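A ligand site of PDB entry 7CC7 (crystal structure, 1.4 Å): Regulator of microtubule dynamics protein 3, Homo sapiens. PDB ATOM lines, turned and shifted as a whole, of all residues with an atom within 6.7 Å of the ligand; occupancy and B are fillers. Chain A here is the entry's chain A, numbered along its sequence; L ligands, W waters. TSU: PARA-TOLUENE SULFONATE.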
ATOM      1  N   ALA A  98      19.727 -15.696  37.375  1.00  0.00           N
ATOM      2  CA  ALA A  98      20.537 -15.330  36.189  1.00  0.00           C
ATOM      3  C   ALA A  98      21.487 -14.199  36.563  1.00  0.00           C
ATOM      4  O   ALA A  98      22.457 -13.984  35.786  1.00  0.00           O
ATOM      5  CB  ALA A  98      19.627 -14.951  35.077  1.00  0.00           C
ATOM      6  N   GLU A  99      21.270 -13.490  37.662  1.00  0.00           N
ATOM      7  CA  GLU A  99      22.243 -12.524  38.201  1.00  0.00           C
ATOM      8  C   GLU A  99      23.472 -13.426  38.453  1.00  0.00           C
ATOM      9  O   GLU A  99      24.551 -12.896  38.556  1.00  0.00           O
ATOM     10  CB  GLU A  99      21.737 -11.782  39.450  1.00  0.00           C
ATOM     11  CG  GLU A  99      20.441 -10.980  39.291  1.00  0.00           C
ATOM     12  CD  GLU A  99      19.847 -10.356  40.555  1.00  0.00           C
ATOM     13  OE1 GLU A  99      18.562 -10.184  40.626  1.00  0.00           O
ATOM     14  OE2 GLU A  99      20.639 -10.053  41.477  1.00  0.00           O
ATOM     15  N   SER A 102      26.632 -16.006  33.359  1.00  0.00           N
ATOM     16  CA  SER A 102      27.206 -16.030  31.978  1.00  0.00           C
ATOM     17  C   SER A 102      26.172 -15.479  30.977  1.00  0.00           C
ATOM     18  O   SER A 102      24.972 -15.609  31.213  1.00  0.00           O
ATOM     19  CB  SER A 102      27.675 -17.422  31.576  1.00  0.00           C
ATOM     20  OG  SER A 102      26.639 -18.210  31.003  1.00  0.00           O
ATOM     21  N   ILE A 103      26.619 -14.913  29.848  1.00  0.00           N
ATOM     22  CA  ILE A 103      25.698 -14.321  28.837  1.00  0.00           C
ATOM     23  C   ILE A 103      24.774 -15.419  28.298  1.00  0.00           C
ATOM     24  O   ILE A 103      23.566 -15.175  28.117  1.00  0.00           O
ATOM     25  CB  ILE A 103      26.485 -13.573  27.746  1.00  0.00           C
ATOM     26  CG1 ILE A 103      25.591 -12.706  26.849  1.00  0.00           C
ATOM     27  CG2 ILE A 103      27.327 -14.558  26.927  1.00  0.00           C
ATOM     28  CD1 ILE A 103      24.684 -11.712  27.600  1.00  0.00           C
ATOM     29  N   ARG A 106      22.180 -16.038  30.965  1.00  0.00           N
ATOM     30  CA  ARG A 106      21.302 -14.846  31.072  1.00  0.00           C
ATOM     31  C   ARG A 106      20.344 -14.860  29.879  1.00  0.00           C
ATOM     32  O   ARG A 106      19.212 -14.357  30.033  1.00  0.00           O
ATOM     33  CB  ARG A 106      22.095 -13.541  31.195  1.00  0.00           C
ATOM     34  CG  ARG A 106      22.733 -13.299  32.562  1.00  0.00           C
ATOM     35  CD  ARG A 106      23.509 -12.000  32.716  1.00  0.00           C
ATOM     36  NE  ARG A 106      24.836 -12.126  32.096  1.00  0.00           N
ATOM     37  CZ  ARG A 106      25.359 -11.323  31.173  1.00  0.00           C
ATOM     38  NH1 ARG A 106      26.561 -11.606  30.704  1.00  0.00           N
ATOM     39  NH2 ARG A 106      24.722 -10.260  30.708  1.00  0.00           N
ATOM     40  N   ILE A 107      20.814 -15.249  28.689  1.00  0.00           N
ATOM     41  CA  ILE A 107      19.929 -15.206  27.497  1.00  0.00           C
ATOM     42  C   ILE A 107      18.826 -16.236  27.653  1.00  0.00           C
ATOM     43  O   ILE A 107      17.654 -15.891  27.411  1.00  0.00           O
ATOM     44  CB  ILE A 107      20.711 -15.382  26.182  1.00  0.00           C
ATOM     45  CG1 ILE A 107      21.518 -14.113  25.896  1.00  0.00           C
ATOM     46  CG2 ILE A 107      19.779 -15.734  25.030  1.00  0.00           C
ATOM     47  CD1 ILE A 107      22.690 -14.346  24.961  1.00  0.00           C
ATOM     48  N   GLN A 108      19.166 -17.465  28.026  1.00  0.00           N
ATOM     49  CA  GLN A 108      18.139 -18.531  28.112  1.00  0.00           C
ATOM     50  C   GLN A 108      17.159 -18.172  29.247  1.00  0.00           C
ATOM     51  O   GLN A 108      15.940 -18.345  29.036  1.00  0.00           O
ATOM     52  CB  GLN A 108      18.759 -19.918  28.326  1.00  0.00           C
ATOM     53  CG  GLN A 108      19.506 -20.457  27.117  1.00  0.00           C
ATOM     54  CD  GLN A 108      18.590 -20.866  25.980  1.00  0.00           C
ATOM     55  OE1 GLN A 108      17.367 -20.937  26.121  1.00  0.00           O
ATOM     56  NE2 GLN A 108      19.183 -21.130  24.822  1.00  0.00           N
ATOM     57  N   SER A 109      17.674 -17.685  30.365  1.00  0.00           N
ATOM     58  CA  SER A 109      16.859 -17.206  31.502  1.00  0.00           C
ATOM     59  C   SER A 109      15.995 -16.047  31.079  1.00  0.00           C
ATOM     60  O   SER A 109      14.817 -16.039  31.402  1.00  0.00           O
ATOM     61  CB  SER A 109      17.707 -16.837  32.656  1.00  0.00           C
ATOM     62  OG  SER A 109      18.409 -18.009  33.037  1.00  0.00           O
ATOM     63  N   GLY A 110      16.538 -15.149  30.256  1.00  0.00           N
ATOM     64  CA  GLY A 110      15.776 -13.977  29.817  1.00  0.00           C
ATOM     65  C   GLY A 110      14.638 -14.360  28.928  1.00  0.00           C
ATOM     66  O   GLY A 110      13.525 -13.786  29.034  1.00  0.00           O
ATOM     67  N   PHE A 111      14.815 -15.369  28.071  1.00  0.00           N
ATOM     68  CA  PHE A 111      13.715 -15.877  27.212  1.00  0.00           C
ATOM     69  C   PHE A 111      12.608 -16.445  28.109  1.00  0.00           C
ATOM     70  O   PHE A 111      11.393 -16.178  27.977  1.00  0.00           O
ATOM     71  CB  PHE A 111      14.238 -16.922  26.222  1.00  0.00           C
ATOM     72  CG  PHE A 111      13.157 -17.624  25.452  1.00  0.00           C
ATOM     73  CD1 PHE A 111      12.624 -17.039  24.314  1.00  0.00           C
ATOM     74  CD2 PHE A 111      12.646 -18.834  25.900  1.00  0.00           C
ATOM     75  CE1 PHE A 111      11.598 -17.677  23.615  1.00  0.00           C
ATOM     76  CE2 PHE A 111      11.616 -19.462  25.211  1.00  0.00           C
ATOM     77  CZ  PHE A 111      11.092 -18.872  24.072  1.00  0.00           C
ATOM     78  N   PHE A 113      12.016 -15.904  31.362  1.00  0.00           N
ATOM     79  CA  PHE A 113      11.459 -14.759  32.113  1.00  0.00           C
ATOM     80  C   PHE A 113      10.320 -14.109  31.318  1.00  0.00           C
ATOM     81  O   PHE A 113       9.218 -13.920  31.811  1.00  0.00           O
ATOM     82  CB  PHE A 113      12.554 -13.764  32.433  1.00  0.00           C
ATOM     83  CG  PHE A 113      12.110 -12.685  33.376  1.00  0.00           C
ATOM     84  CD1 PHE A 113      11.367 -11.605  32.915  1.00  0.00           C
ATOM     85  CD2 PHE A 113      12.531 -12.701  34.696  1.00  0.00           C
ATOM     86  CE1 PHE A 113      11.003 -10.615  33.803  1.00  0.00           C
ATOM     87  CE2 PHE A 113      12.190 -11.690  35.571  1.00  0.00           C
ATOM     88  CZ  PHE A 113      11.419 -10.644  35.124  1.00  0.00           C
ATOM     89  N   LYS A 114      10.598 -13.775  30.057  1.00  0.00           N
ATOM     90  CA  LYS A 114       9.607 -13.048  29.218  1.00  0.00           C
ATOM     91  C   LYS A 114       8.361 -13.884  29.010  1.00  0.00           C
ATOM     92  O   LYS A 114       7.216 -13.398  29.176  1.00  0.00           O
ATOM     93  CB  LYS A 114      10.293 -12.752  27.883  1.00  0.00           C
ATOM     94  CG  LYS A 114       9.399 -12.084  26.834  1.00  0.00           C
ATOM     95  CD  LYS A 114       8.928 -10.762  27.343  1.00  0.00           C
ATOM     96  CE  LYS A 114       8.496  -9.784  26.254  1.00  0.00           C
ATOM     97  NZ  LYS A 114       7.512 -10.403  25.391  1.00  0.00           N
ATOM     98  N   TRP A 137      12.746  -5.846  32.380  1.00  0.00           N
ATOM     99  CA  TRP A 137      13.204  -6.783  31.332  1.00  0.00           C
ATOM    100  C   TRP A 137      13.406  -6.002  30.023  1.00  0.00           C
ATOM    101  O   TRP A 137      14.424  -6.128  29.406  1.00  0.00           O
ATOM    102  CB  TRP A 137      12.253  -7.965  31.174  1.00  0.00           C
ATOM    103  CG  TRP A 137      12.651  -8.981  30.167  1.00  0.00           C
ATOM    104  CD1 TRP A 137      13.311 -10.160  30.410  1.00  0.00           C
ATOM    105  CD2 TRP A 137      12.352  -8.982  28.752  1.00  0.00           C
ATOM    106  NE1 TRP A 137      13.459 -10.851  29.252  1.00  0.00           N
ATOM    107  CE2 TRP A 137      12.916 -10.153  28.205  1.00  0.00           C
ATOM    108  CE3 TRP A 137      11.717  -8.068  27.910  1.00  0.00           C
ATOM    109  CZ2 TRP A 137      12.814 -10.476  26.862  1.00  0.00           C
ATOM    110  CZ3 TRP A 137      11.606  -8.396  26.568  1.00  0.00           C
ATOM    111  CH2 TRP A 137      12.168  -9.554  26.060  1.00  0.00           C
ATOM    112  N   GLN A 140      16.388  -3.670  30.163  1.00  0.00           N
ATOM    113  CA  GLN A 140      17.654  -4.445  30.110  1.00  0.00           C
ATOM    114  C   GLN A 140      17.857  -4.899  28.676  1.00  0.00           C
ATOM    115  O   GLN A 140      19.041  -4.827  28.204  1.00  0.00           O
ATOM    116  CB  GLN A 140      17.549  -5.650  31.063  1.00  0.00           C
ATOM    117  CG  GLN A 140      17.641  -5.378  32.521  1.00  0.00           C
ATOM    118  CD  GLN A 140      17.270  -6.642  33.280  1.00  0.00           C
ATOM    119  OE1 GLN A 140      16.432  -6.627  34.120  1.00  0.00           O
ATOM    120  NE2 GLN A 140      17.830  -7.790  32.922  1.00  0.00           N
ATOM    121  N   VAL A 141      16.876  -5.436  28.016  1.00  0.00           N
ATOM    122  CA  VAL A 141      17.035  -5.950  26.640  1.00  0.00           C
ATOM    123  C   VAL A 141      17.427  -4.787  25.728  1.00  0.00           C
ATOM    124  O   VAL A 141      18.353  -4.971  24.890  1.00  0.00           O
ATOM    125  CB  VAL A 141      15.798  -6.715  26.154  1.00  0.00           C
ATOM    126  CG1 VAL A 141      15.845  -6.936  24.654  1.00  0.00           C
ATOM    127  CG2 VAL A 141      15.662  -8.037  26.898  1.00  0.00           C
ATOM    128  N   LEU A 144      21.178  -4.049  25.935  1.00  0.00           N
ATOM    129  CA  LEU A 144      22.184  -5.089  25.576  1.00  0.00           C
ATOM    130  C   LEU A 144      23.137  -4.445  24.568  1.00  0.00           C
ATOM    131  O   LEU A 144      22.706  -3.672  23.690  1.00  0.00           O
ATOM    132  CB  LEU A 144      21.532  -6.328  25.008  1.00  0.00           C
ATOM    133  CG  LEU A 144      20.759  -7.139  26.054  1.00  0.00           C
ATOM    134  CD1 LEU A 144      20.008  -8.213  25.355  1.00  0.00           C
ATOM    135  CD2 LEU A 144      21.637  -7.689  27.163  1.00  0.00           C
ATOM    136  N   GLU A 148      26.124  -8.653  22.602  1.00  0.00           N
ATOM    137  CA  GLU A 148      25.180  -9.451  23.403  1.00  0.00           C
ATOM    138  C   GLU A 148      23.919  -9.740  22.611  1.00  0.00           C
ATOM    139  O   GLU A 148      23.389 -10.848  22.609  1.00  0.00           O
ATOM    140  CB  GLU A 148      24.827  -8.746  24.689  1.00  0.00           C
ATOM    141  CG  GLU A 148      25.959  -8.666  25.687  1.00  0.00           C
ATOM    142  CD  GLU A 148      25.689  -7.753  26.879  1.00  0.00           C
ATOM    143  OE1 GLU A 148      25.074  -6.680  26.715  1.00  0.00           O
ATOM    144  OE2 GLU A 148      26.083  -8.105  28.021  1.00  0.00           O
ATOM    145  N   ALA A 152      22.505 -13.371  21.519  1.00  0.00           N
ATOM    146  CA  ALA A 152      21.119 -13.784  21.790  1.00  0.00           C
ATOM    147  C   ALA A 152      20.403 -14.199  20.514  1.00  0.00           C
ATOM    148  O   ALA A 152      19.644 -15.192  20.521  1.00  0.00           O
ATOM    149  CB  ALA A 152      20.388 -12.636  22.468  1.00  0.00           C
ATOM    150  N   LEU A 156      18.691 -17.987  20.365  1.00  0.00           N
ATOM    151  CA  LEU A 156      17.203 -18.060  20.498  1.00  0.00           C
ATOM    152  C   LEU A 156      16.555 -18.329  19.124  1.00  0.00           C
ATOM    153  O   LEU A 156      17.243 -18.052  18.102  1.00  0.00           O
ATOM    154  CB  LEU A 156      16.695 -16.757  21.131  1.00  0.00           C
ATOM    155  CG  LEU A 156      17.179 -16.482  22.551  1.00  0.00           C
ATOM    156  CD1 LEU A 156      16.735 -15.107  23.014  1.00  0.00           C
ATOM    157  CD2 LEU A 156      16.699 -17.561  23.529  1.00  0.00           C
ATOM    158  N   LEU A 160      15.957 -10.420  19.579  1.00  0.00           N
ATOM    159  CA  LEU A 160      15.398  -9.529  20.626  1.00  0.00           C
ATOM    160  C   LEU A 160      15.207  -8.136  20.050  1.00  0.00           C
ATOM    161  O   LEU A 160      16.041  -7.676  19.246  1.00  0.00           O
ATOM    162  CB  LEU A 160      16.363  -9.459  21.803  1.00  0.00           C
ATOM    163  CG  LEU A 160      16.561 -10.757  22.581  1.00  0.00           C
ATOM    164  CD1 LEU A 160      17.611 -10.555  23.661  1.00  0.00           C
ATOM    165  CD2 LEU A 160      15.248 -11.244  23.178  1.00  0.00           C
HETATM  166  S   TSU L   1      20.447  -9.592  30.845  1.00  0.00           S
HETATM  167  O1  TSU L   1      21.793  -9.833  30.355  1.00  0.00           O
HETATM  168  O2  TSU L   1      20.209  -8.119  31.038  1.00  0.00           O
HETATM  169  O3  TSU L   1      20.248 -10.343  32.091  1.00  0.00           O
HETATM  170  C1  TSU L   1      19.323 -10.255  29.670  1.00  0.00           C
HETATM  171  C2  TSU L   1      19.801 -10.975  28.591  1.00  0.00           C
HETATM  172  C3  TSU L   1      18.903 -11.503  27.675  1.00  0.00           C
HETATM  173  C4  TSU L   1      17.527 -11.335  27.831  1.00  0.00           C
HETATM  174  C5  TSU L   1      17.095 -10.613  28.938  1.00  0.00           C
HETATM  175  C6  TSU L   1      17.962 -10.109  29.877  1.00  0.00           C
HETATM  176  C7  TSU L   1      16.536 -11.910  26.863  1.00  0.00           C
HETATM  177  O   HOH W   1      20.990 -10.156  34.745  1.00  0.00           O
HETATM  178  O   HOH W   2      18.775 -12.862  32.223  1.00  0.00           O
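NE2 of Gln 140 is in hydrogen-bond range of O2 of the ligand. O1 of the ligand lies within salt-bridge range of NH2 of Arg 106.
The indole nitrogen of Trp 137 lies within hydrogen-bond range of the backbone carbonyl oxygen of Gly 110 (2.9 Å). The guanidinium group of Arg 106 is in salt-bridge range of the side-chain carboxylate of Glu 148 (3.7 Å).
Ile 107 touches the ligand (CA to C3, 3.8 Å). CA of Gly 110 touches C7 of the ligand (3.7 Å). NE1 of Trp 137 touches C5 of the ligand, 3.7 Å away. Val 141 touches the ligand (CG2 to C5, 3.6 Å). CD2 of Leu 144 touches O1 of the ligand, 3.8 Å away. CD1 of Leu 160 touches C7 of the ligand, at 3.6 Å. Hydrophobic or aromatic side chains that line the ligand: Trp 137, Val 141, Leu 144 and Leu 160.
Water W2 bridges O of Arg 106 (2.7 Å) and O3 of the ligand (2.9 Å).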
